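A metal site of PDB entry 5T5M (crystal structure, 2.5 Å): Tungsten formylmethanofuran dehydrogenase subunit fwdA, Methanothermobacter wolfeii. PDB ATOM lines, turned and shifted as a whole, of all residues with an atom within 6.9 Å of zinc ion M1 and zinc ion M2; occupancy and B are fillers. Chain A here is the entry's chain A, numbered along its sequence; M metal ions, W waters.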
ATOM      1  N   HIS A  57      32.700  27.822 -29.830  1.00  0.00           N
ATOM      2  CA  HIS A  57      31.325  27.728 -29.307  1.00  0.00           C
ATOM      3  C   HIS A  57      31.041  26.296 -28.850  1.00  0.00           C
ATOM      4  O   HIS A  57      30.705  25.432 -29.663  1.00  0.00           O
ATOM      5  CB  HIS A  57      30.325  28.158 -30.367  1.00  0.00           C
ATOM      6  CG  HIS A  57      28.961  28.404 -29.829  1.00  0.00           C
ATOM      7  ND1 HIS A  57      28.496  29.676 -29.550  1.00  0.00           N
ATOM      8  CD2 HIS A  57      27.954  27.561 -29.512  1.00  0.00           C
ATOM      9  CE1 HIS A  57      27.257  29.596 -29.090  1.00  0.00           C
ATOM     10  NE2 HIS A  57      26.906  28.326 -29.050  1.00  0.00           N
ATOM     11  N   SER A  58      31.131  26.074 -27.545  1.00  0.00           N
ATOM     12  CA  SER A  58      30.876  24.775 -26.948  1.00  0.00           C
ATOM     13  C   SER A  58      30.249  24.970 -25.576  1.00  0.00           C
ATOM     14  O   SER A  58      30.464  25.993 -24.929  1.00  0.00           O
ATOM     15  CB  SER A  58      32.172  23.973 -26.856  1.00  0.00           C
ATOM     16  OG  SER A  58      31.934  22.609 -26.575  1.00  0.00           O
ATOM     17  N   HIS A  59      29.455  24.003 -25.143  1.00  0.00           N
ATOM     18  CA  HIS A  59      28.837  24.062 -23.821  1.00  0.00           C
ATOM     19  C   HIS A  59      29.515  23.021 -22.943  1.00  0.00           C
ATOM     20  O   HIS A  59      29.153  21.848 -22.946  1.00  0.00           O
ATOM     21  CB  HIS A  59      27.333  23.850 -23.927  1.00  0.00           C
ATOM     22  CG  HIS A  59      26.626  24.951 -24.651  1.00  0.00           C
ATOM     23  ND1 HIS A  59      26.160  26.088 -24.021  1.00  0.00           N
ATOM     24  CD2 HIS A  59      26.348  25.110 -25.967  1.00  0.00           C
ATOM     25  CE1 HIS A  59      25.608  26.889 -24.911  1.00  0.00           C
ATOM     26  NE2 HIS A  59      25.705  26.318 -26.101  1.00  0.00           N
ATOM     27  N   ALA A 115      30.212  28.884 -24.049  1.00  0.00           N
ATOM     28  CA  ALA A 115      29.441  29.779 -24.897  1.00  0.00           C
ATOM     29  C   ALA A 115      28.340  30.564 -24.182  1.00  0.00           C
ATOM     30  O   ALA A 115      27.865  31.551 -24.738  1.00  0.00           O
ATOM     31  CB  ALA A 115      28.817  28.980 -26.039  1.00  0.00           C
ATOM     32  N   ALA A 116      27.907  30.149 -22.971  1.00  0.00           N
ATOM     33  CA  ALA A 116      26.764  30.815 -22.334  1.00  0.00           C
ATOM     34  C   ALA A 116      26.871  30.716 -20.819  1.00  0.00           C
ATOM     35  O   ALA A 116      26.426  29.735 -20.224  1.00  0.00           O
ATOM     36  CB  ALA A 116      25.467  30.204 -22.836  1.00  0.00           C
ATOM     37  N   KCX A 178      27.713  37.767 -25.207  1.00  0.00           N
ATOM     38  CA  KCX A 178      26.837  36.732 -25.811  1.00  0.00           C
ATOM     39  CB  KCX A 178      27.054  35.403 -25.076  1.00  0.00           C
ATOM     40  CG  KCX A 178      26.086  34.351 -25.598  1.00  0.00           C
ATOM     41  CD  KCX A 178      26.563  33.941 -26.984  1.00  0.00           C
ATOM     42  CE  KCX A 178      25.682  32.876 -27.610  1.00  0.00           C
ATOM     43  NZ  KCX A 178      25.795  31.612 -26.918  1.00  0.00           N
ATOM     44  C   KCX A 178      25.377  37.134 -25.730  1.00  0.00           C
ATOM     45  O   KCX A 178      24.912  37.604 -24.661  1.00  0.00           O
ATOM     46  CX  KCX A 178      24.938  30.648 -27.216  1.00  0.00           C
ATOM     47  OQ1 KCX A 178      24.039  30.821 -28.026  1.00  0.00           O
ATOM     48  OQ2 KCX A 178      25.061  29.443 -26.649  1.00  0.00           O
ATOM     49  N   ILE A 179      24.654  36.995 -26.840  1.00  0.00           N
ATOM     50  CA  ILE A 179      23.253  37.402 -26.930  1.00  0.00           C
ATOM     51  C   ILE A 179      22.409  36.205 -27.366  1.00  0.00           C
ATOM     52  O   ILE A 179      22.556  35.728 -28.490  1.00  0.00           O
ATOM     53  CB  ILE A 179      23.077  38.572 -27.929  1.00  0.00           C
ATOM     54  CG1 ILE A 179      24.124  39.658 -27.676  1.00  0.00           C
ATOM     55  CG2 ILE A 179      21.674  39.135 -27.837  1.00  0.00           C
ATOM     56  CD1 ILE A 179      24.104  40.786 -28.692  1.00  0.00           C
ATOM     57  N   VAL A 180      21.522  35.724 -26.493  1.00  0.00           N
ATOM     58  CA  VAL A 180      20.707  34.547 -26.768  1.00  0.00           C
ATOM     59  C   VAL A 180      19.238  34.955 -26.706  1.00  0.00           C
ATOM     60  O   VAL A 180      18.741  35.340 -25.643  1.00  0.00           O
ATOM     61  CB  VAL A 180      20.999  33.409 -25.778  1.00  0.00           C
ATOM     62  CG1 VAL A 180      19.990  32.276 -25.945  1.00  0.00           C
ATOM     63  CG2 VAL A 180      22.408  32.896 -25.987  1.00  0.00           C
ATOM     64  N   HIS A 229      28.237  37.981 -30.067  1.00  0.00           N
ATOM     65  CA  HIS A 229      28.062  36.570 -30.403  1.00  0.00           C
ATOM     66  C   HIS A 229      26.553  36.329 -30.361  1.00  0.00           C
ATOM     67  O   HIS A 229      25.971  36.263 -29.271  1.00  0.00           O
ATOM     68  CB  HIS A 229      28.814  35.729 -29.380  1.00  0.00           C
ATOM     69  CG  HIS A 229      29.213  34.369 -29.854  1.00  0.00           C
ATOM     70  ND1 HIS A 229      30.506  34.068 -30.205  1.00  0.00           N
ATOM     71  CD2 HIS A 229      28.509  33.217 -29.979  1.00  0.00           C
ATOM     72  CE1 HIS A 229      30.576  32.794 -30.546  1.00  0.00           C
ATOM     73  NE2 HIS A 229      29.384  32.256 -30.422  1.00  0.00           N
ATOM     74  N   LEU A 230      25.914  36.208 -31.521  1.00  0.00           N
ATOM     75  CA  LEU A 230      24.462  36.282 -31.606  1.00  0.00           C
ATOM     76  C   LEU A 230      23.827  34.928 -31.898  1.00  0.00           C
ATOM     77  O   LEU A 230      24.171  34.267 -32.889  1.00  0.00           O
ATOM     78  CB  LEU A 230      24.017  37.298 -32.662  1.00  0.00           C
ATOM     79  CG  LEU A 230      22.493  37.434 -32.801  1.00  0.00           C
ATOM     80  CD1 LEU A 230      21.854  37.793 -31.466  1.00  0.00           C
ATOM     81  CD2 LEU A 230      22.141  38.482 -33.856  1.00  0.00           C
ATOM     82  N   HIS A 231      22.886  34.540 -31.026  1.00  0.00           N
ATOM     83  CA  HIS A 231      21.975  33.403 -31.185  1.00  0.00           C
ATOM     84  C   HIS A 231      20.592  34.023 -31.420  1.00  0.00           C
ATOM     85  O   HIS A 231      19.993  34.580 -30.502  1.00  0.00           O
ATOM     86  CB  HIS A 231      22.065  32.526 -29.931  1.00  0.00           C
ATOM     87  CG  HIS A 231      20.901  31.618 -29.646  1.00  0.00           C
ATOM     88  ND1 HIS A 231      21.073  30.358 -29.115  1.00  0.00           N
ATOM     89  CD2 HIS A 231      19.551  31.808 -29.724  1.00  0.00           C
ATOM     90  CE1 HIS A 231      19.897  29.795 -28.904  1.00  0.00           C
ATOM     91  NE2 HIS A 231      18.957  30.652 -29.270  1.00  0.00           N
ATOM     92  N   CYS A 232      20.103  33.945 -32.660  1.00  0.00           N
ATOM     93  CA  CYS A 232      18.974  34.766 -33.095  1.00  0.00           C
ATOM     94  C   CYS A 232      17.662  34.351 -32.429  1.00  0.00           C
ATOM     95  O   CYS A 232      17.506  33.244 -31.929  1.00  0.00           O
ATOM     96  CB  CYS A 232      18.792  34.689 -34.612  1.00  0.00           C
ATOM     97  SG  CYS A 232      20.078  35.471 -35.571  1.00  0.00           S
ATOM     98  N   LEU A 235      14.630  30.633 -32.965  1.00  0.00           N
ATOM     99  CA  LEU A 235      15.424  29.447 -33.283  1.00  0.00           C
ATOM    100  C   LEU A 235      14.534  28.228 -33.550  1.00  0.00           C
ATOM    101  O   LEU A 235      13.571  27.950 -32.819  1.00  0.00           O
ATOM    102  CB  LEU A 235      16.389  29.140 -32.133  1.00  0.00           C
ATOM    103  CG  LEU A 235      17.382  27.985 -32.383  1.00  0.00           C
ATOM    104  CD1 LEU A 235      18.665  28.242 -31.647  1.00  0.00           C
ATOM    105  CD2 LEU A 235      16.819  26.626 -31.965  1.00  0.00           C
ATOM    106  N   THR A 270      26.006  32.504 -34.417  1.00  0.00           N
ATOM    107  CA  THR A 270      26.337  31.132 -34.058  1.00  0.00           C
ATOM    108  C   THR A 270      25.223  30.156 -34.462  1.00  0.00           C
ATOM    109  O   THR A 270      24.049  30.533 -34.620  1.00  0.00           O
ATOM    110  CB  THR A 270      26.614  31.018 -32.558  1.00  0.00           C
ATOM    111  OG1 THR A 270      26.993  29.681 -32.238  1.00  0.00           O
ATOM    112  CG2 THR A 270      25.388  31.422 -31.739  1.00  0.00           C
ATOM    113  N   HIS A 271      25.624  28.896 -34.608  1.00  0.00           N
ATOM    114  CA  HIS A 271      24.787  27.788 -35.078  1.00  0.00           C
ATOM    115  C   HIS A 271      23.669  28.234 -36.013  1.00  0.00           C
ATOM    116  O   HIS A 271      22.490  28.070 -35.721  1.00  0.00           O
ATOM    117  CB  HIS A 271      24.208  26.988 -33.894  1.00  0.00           C
ATOM    118  CG  HIS A 271      23.561  27.816 -32.823  1.00  0.00           C
ATOM    119  ND1 HIS A 271      22.354  28.445 -32.991  1.00  0.00           N
ATOM    120  CD2 HIS A 271      23.929  28.051 -31.539  1.00  0.00           C
ATOM    121  CE1 HIS A 271      22.022  29.070 -31.872  1.00  0.00           C
ATOM    122  NE2 HIS A 271      22.963  28.836 -30.977  1.00  0.00           N
ATOM    123  N   HIS A 275      18.808  28.388 -37.879  1.00  0.00           N
ATOM    124  CA  HIS A 275      18.219  29.685 -38.218  1.00  0.00           C
ATOM    125  C   HIS A 275      18.009  29.845 -39.726  1.00  0.00           C
ATOM    126  O   HIS A 275      17.785  30.970 -40.196  1.00  0.00           O
ATOM    127  CB  HIS A 275      19.107  30.796 -37.668  1.00  0.00           C
ATOM    128  CG  HIS A 275      19.306  30.733 -36.193  1.00  0.00           C
ATOM    129  ND1 HIS A 275      18.420  31.300 -35.308  1.00  0.00           N
ATOM    130  CD2 HIS A 275      20.283  30.178 -35.433  1.00  0.00           C
ATOM    131  CE1 HIS A 275      18.840  31.099 -34.068  1.00  0.00           C
ATOM    132  NE2 HIS A 275      19.981  30.429 -34.123  1.00  0.00           N
ATOM    133  N   MET A 317      21.063  22.006 -24.604  1.00  0.00           N
ATOM    134  CA  MET A 317      21.236  22.859 -23.438  1.00  0.00           C
ATOM    135  C   MET A 317      21.560  24.263 -23.938  1.00  0.00           C
ATOM    136  O   MET A 317      22.596  24.498 -24.563  1.00  0.00           O
ATOM    137  CB  MET A 317      22.336  22.333 -22.518  1.00  0.00           C
ATOM    138  CG  MET A 317      23.628  21.911 -23.219  1.00  0.00           C
ATOM    139  SD  MET A 317      24.889  21.302 -22.088  1.00  0.00           S
ATOM    140  CE  MET A 317      24.039  19.968 -21.271  1.00  0.00           C
ATOM    141  N   THR A 318      20.654  25.207 -23.686  1.00  0.00           N
ATOM    142  CA  THR A 318      20.816  26.556 -24.187  1.00  0.00           C
ATOM    143  C   THR A 318      20.274  27.536 -23.157  1.00  0.00           C
ATOM    144  O   THR A 318      19.521  27.166 -22.258  1.00  0.00           O
ATOM    145  CB  THR A 318      20.077  26.777 -25.529  1.00  0.00           C
ATOM    146  OG1 THR A 318      18.663  26.800 -25.308  1.00  0.00           O
ATOM    147  CG2 THR A 318      20.419  25.680 -26.514  1.00  0.00           C
ATOM    148  N   ALA A 319      20.678  28.789 -23.309  1.00  0.00           N
ATOM    149  CA  ALA A 319      20.084  29.881 -22.571  1.00  0.00           C
ATOM    150  C   ALA A 319      18.780  30.342 -23.191  1.00  0.00           C
ATOM    151  O   ALA A 319      18.277  31.416 -22.847  1.00  0.00           O
ATOM    152  CB  ALA A 319      21.083  31.046 -22.481  1.00  0.00           C
ATOM    153  N   ASP A 320      18.227  29.549 -24.114  1.00  0.00           N
ATOM    154  CA  ASP A 320      16.972  29.844 -24.787  1.00  0.00           C
ATOM    155  C   ASP A 320      15.847  29.057 -24.103  1.00  0.00           C
ATOM    156  O   ASP A 320      15.303  28.076 -24.619  1.00  0.00           O
ATOM    157  CB  ASP A 320      17.093  29.516 -26.280  1.00  0.00           C
ATOM    158  CG  ASP A 320      15.975  30.112 -27.114  1.00  0.00           C
ATOM    159  OD1 ASP A 320      14.910  30.443 -26.555  1.00  0.00           O
ATOM    160  OD2 ASP A 320      16.178  30.241 -28.352  1.00  0.00           O
ATOM    161  N   ASP A 385      27.299  23.347 -31.971  1.00  0.00           N
ATOM    162  CA  ASP A 385      26.718  23.932 -30.770  1.00  0.00           C
ATOM    163  C   ASP A 385      26.802  22.921 -29.636  1.00  0.00           C
ATOM    164  O   ASP A 385      25.866  22.760 -28.857  1.00  0.00           O
ATOM    165  CB  ASP A 385      25.265  24.363 -31.008  1.00  0.00           C
ATOM    166  CG  ASP A 385      24.696  25.203 -29.858  1.00  0.00           C
ATOM    167  OD1 ASP A 385      25.488  25.824 -29.114  1.00  0.00           O
ATOM    168  OD2 ASP A 385      23.450  25.260 -29.708  1.00  0.00           O
ATOM    169  N   SER A 386      27.946  22.240 -29.552  1.00  0.00           N
ATOM    170  CA  SER A 386      28.110  21.084 -28.691  1.00  0.00           C
ATOM    171  C   SER A 386      27.452  21.261 -27.320  1.00  0.00           C
ATOM    172  O   SER A 386      27.713  22.236 -26.628  1.00  0.00           O
ATOM    173  CB  SER A 386      29.602  20.781 -28.485  1.00  0.00           C
ATOM    174  OG  SER A 386      29.782  19.562 -27.780  1.00  0.00           O
ATOM    175  N   ASN A 388      24.339  20.442 -28.534  1.00  0.00           N
ATOM    176  CA  ASN A 388      22.972  20.646 -29.022  1.00  0.00           C
ATOM    177  C   ASN A 388      22.719  19.922 -30.346  1.00  0.00           C
ATOM    178  O   ASN A 388      21.692  19.256 -30.517  1.00  0.00           O
ATOM    179  CB  ASN A 388      22.703  22.140 -29.161  1.00  0.00           C
ATOM    180  CG  ASN A 388      22.514  22.825 -27.821  1.00  0.00           C
ATOM    181  OD1 ASN A 388      21.430  22.773 -27.241  1.00  0.00           O
ATOM    182  ND2 ASN A 388      23.565  23.457 -27.322  1.00  0.00           N
HETATM  183 ZN    ZN M   1      22.903  29.259 -28.856  1.00  0.00          ZN
HETATM  184 ZN    ZN M   2      25.310  27.464 -27.780  1.00  0.00          ZN
HETATM  185  O   HOH W   1      23.467  27.466 -28.414  1.00  0.00           O
HETATM  186  O   HOH W   2      22.432  28.895 -25.464  1.00  0.00           O
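ND1 of His 271 sits at hydrogen-bond distance from NE2 of His 275 (3.3 Å). A ring nitrogen (NE2) of His 231 is in hydrogen-bond range of the side-chain carboxylate (OD2) of Asp 320, at 3.0 Å. N of His 59 is in hydrogen-bond range of O of Ser 386, at 2.9 Å. ND1 of His 57 sits at hydrogen-bond distance from NE2 of His 229 (2.9 Å). The side-chain amide nitrogen of Asn 388 lies within hydrogen-bond range of the backbone carbonyl oxygen of Asp 385 (2.9 Å). The side-chain hydroxyl (OG1) of Thr 270 lies within hydrogen-bond range of a ring nitrogen (ND1) of His 57. The backbone NH (N) of His 231 lies within hydrogen-bond range of the backbone carbonyl oxygen (O) of Ile 179 (2.8 Å). O of Ala 115 lies within hydrogen-bond range of NZ of KCX 178 (3.0 Å).
Of the 23 residues printed, 3 come within 4 Å of zinc ion M1.
Along chain A the residues within 4 Å of zinc ion M2 span positions 57 to 385. The nearest printed residue that does not touch zinc ion M2 is His 271 (4.05 Å).
Zinc ion M1 is bound by water W1 (1.9 Å). OQ1 of KCX 178 is bound to zinc ion M1. Zinc ion M1 is bound by a ring nitrogen (ND1) of His 231 (2.2 Å). NE2 of His 271 is bound to zinc ion M1, 2.2 Å away. Zinc ion M1 has four donor atoms within binding distance.
Zinc ion M2 is bound by water W1, NE2 of His 59, OD1 of Asp 385, NE2 of His 57 and OQ2 of KCX 178.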
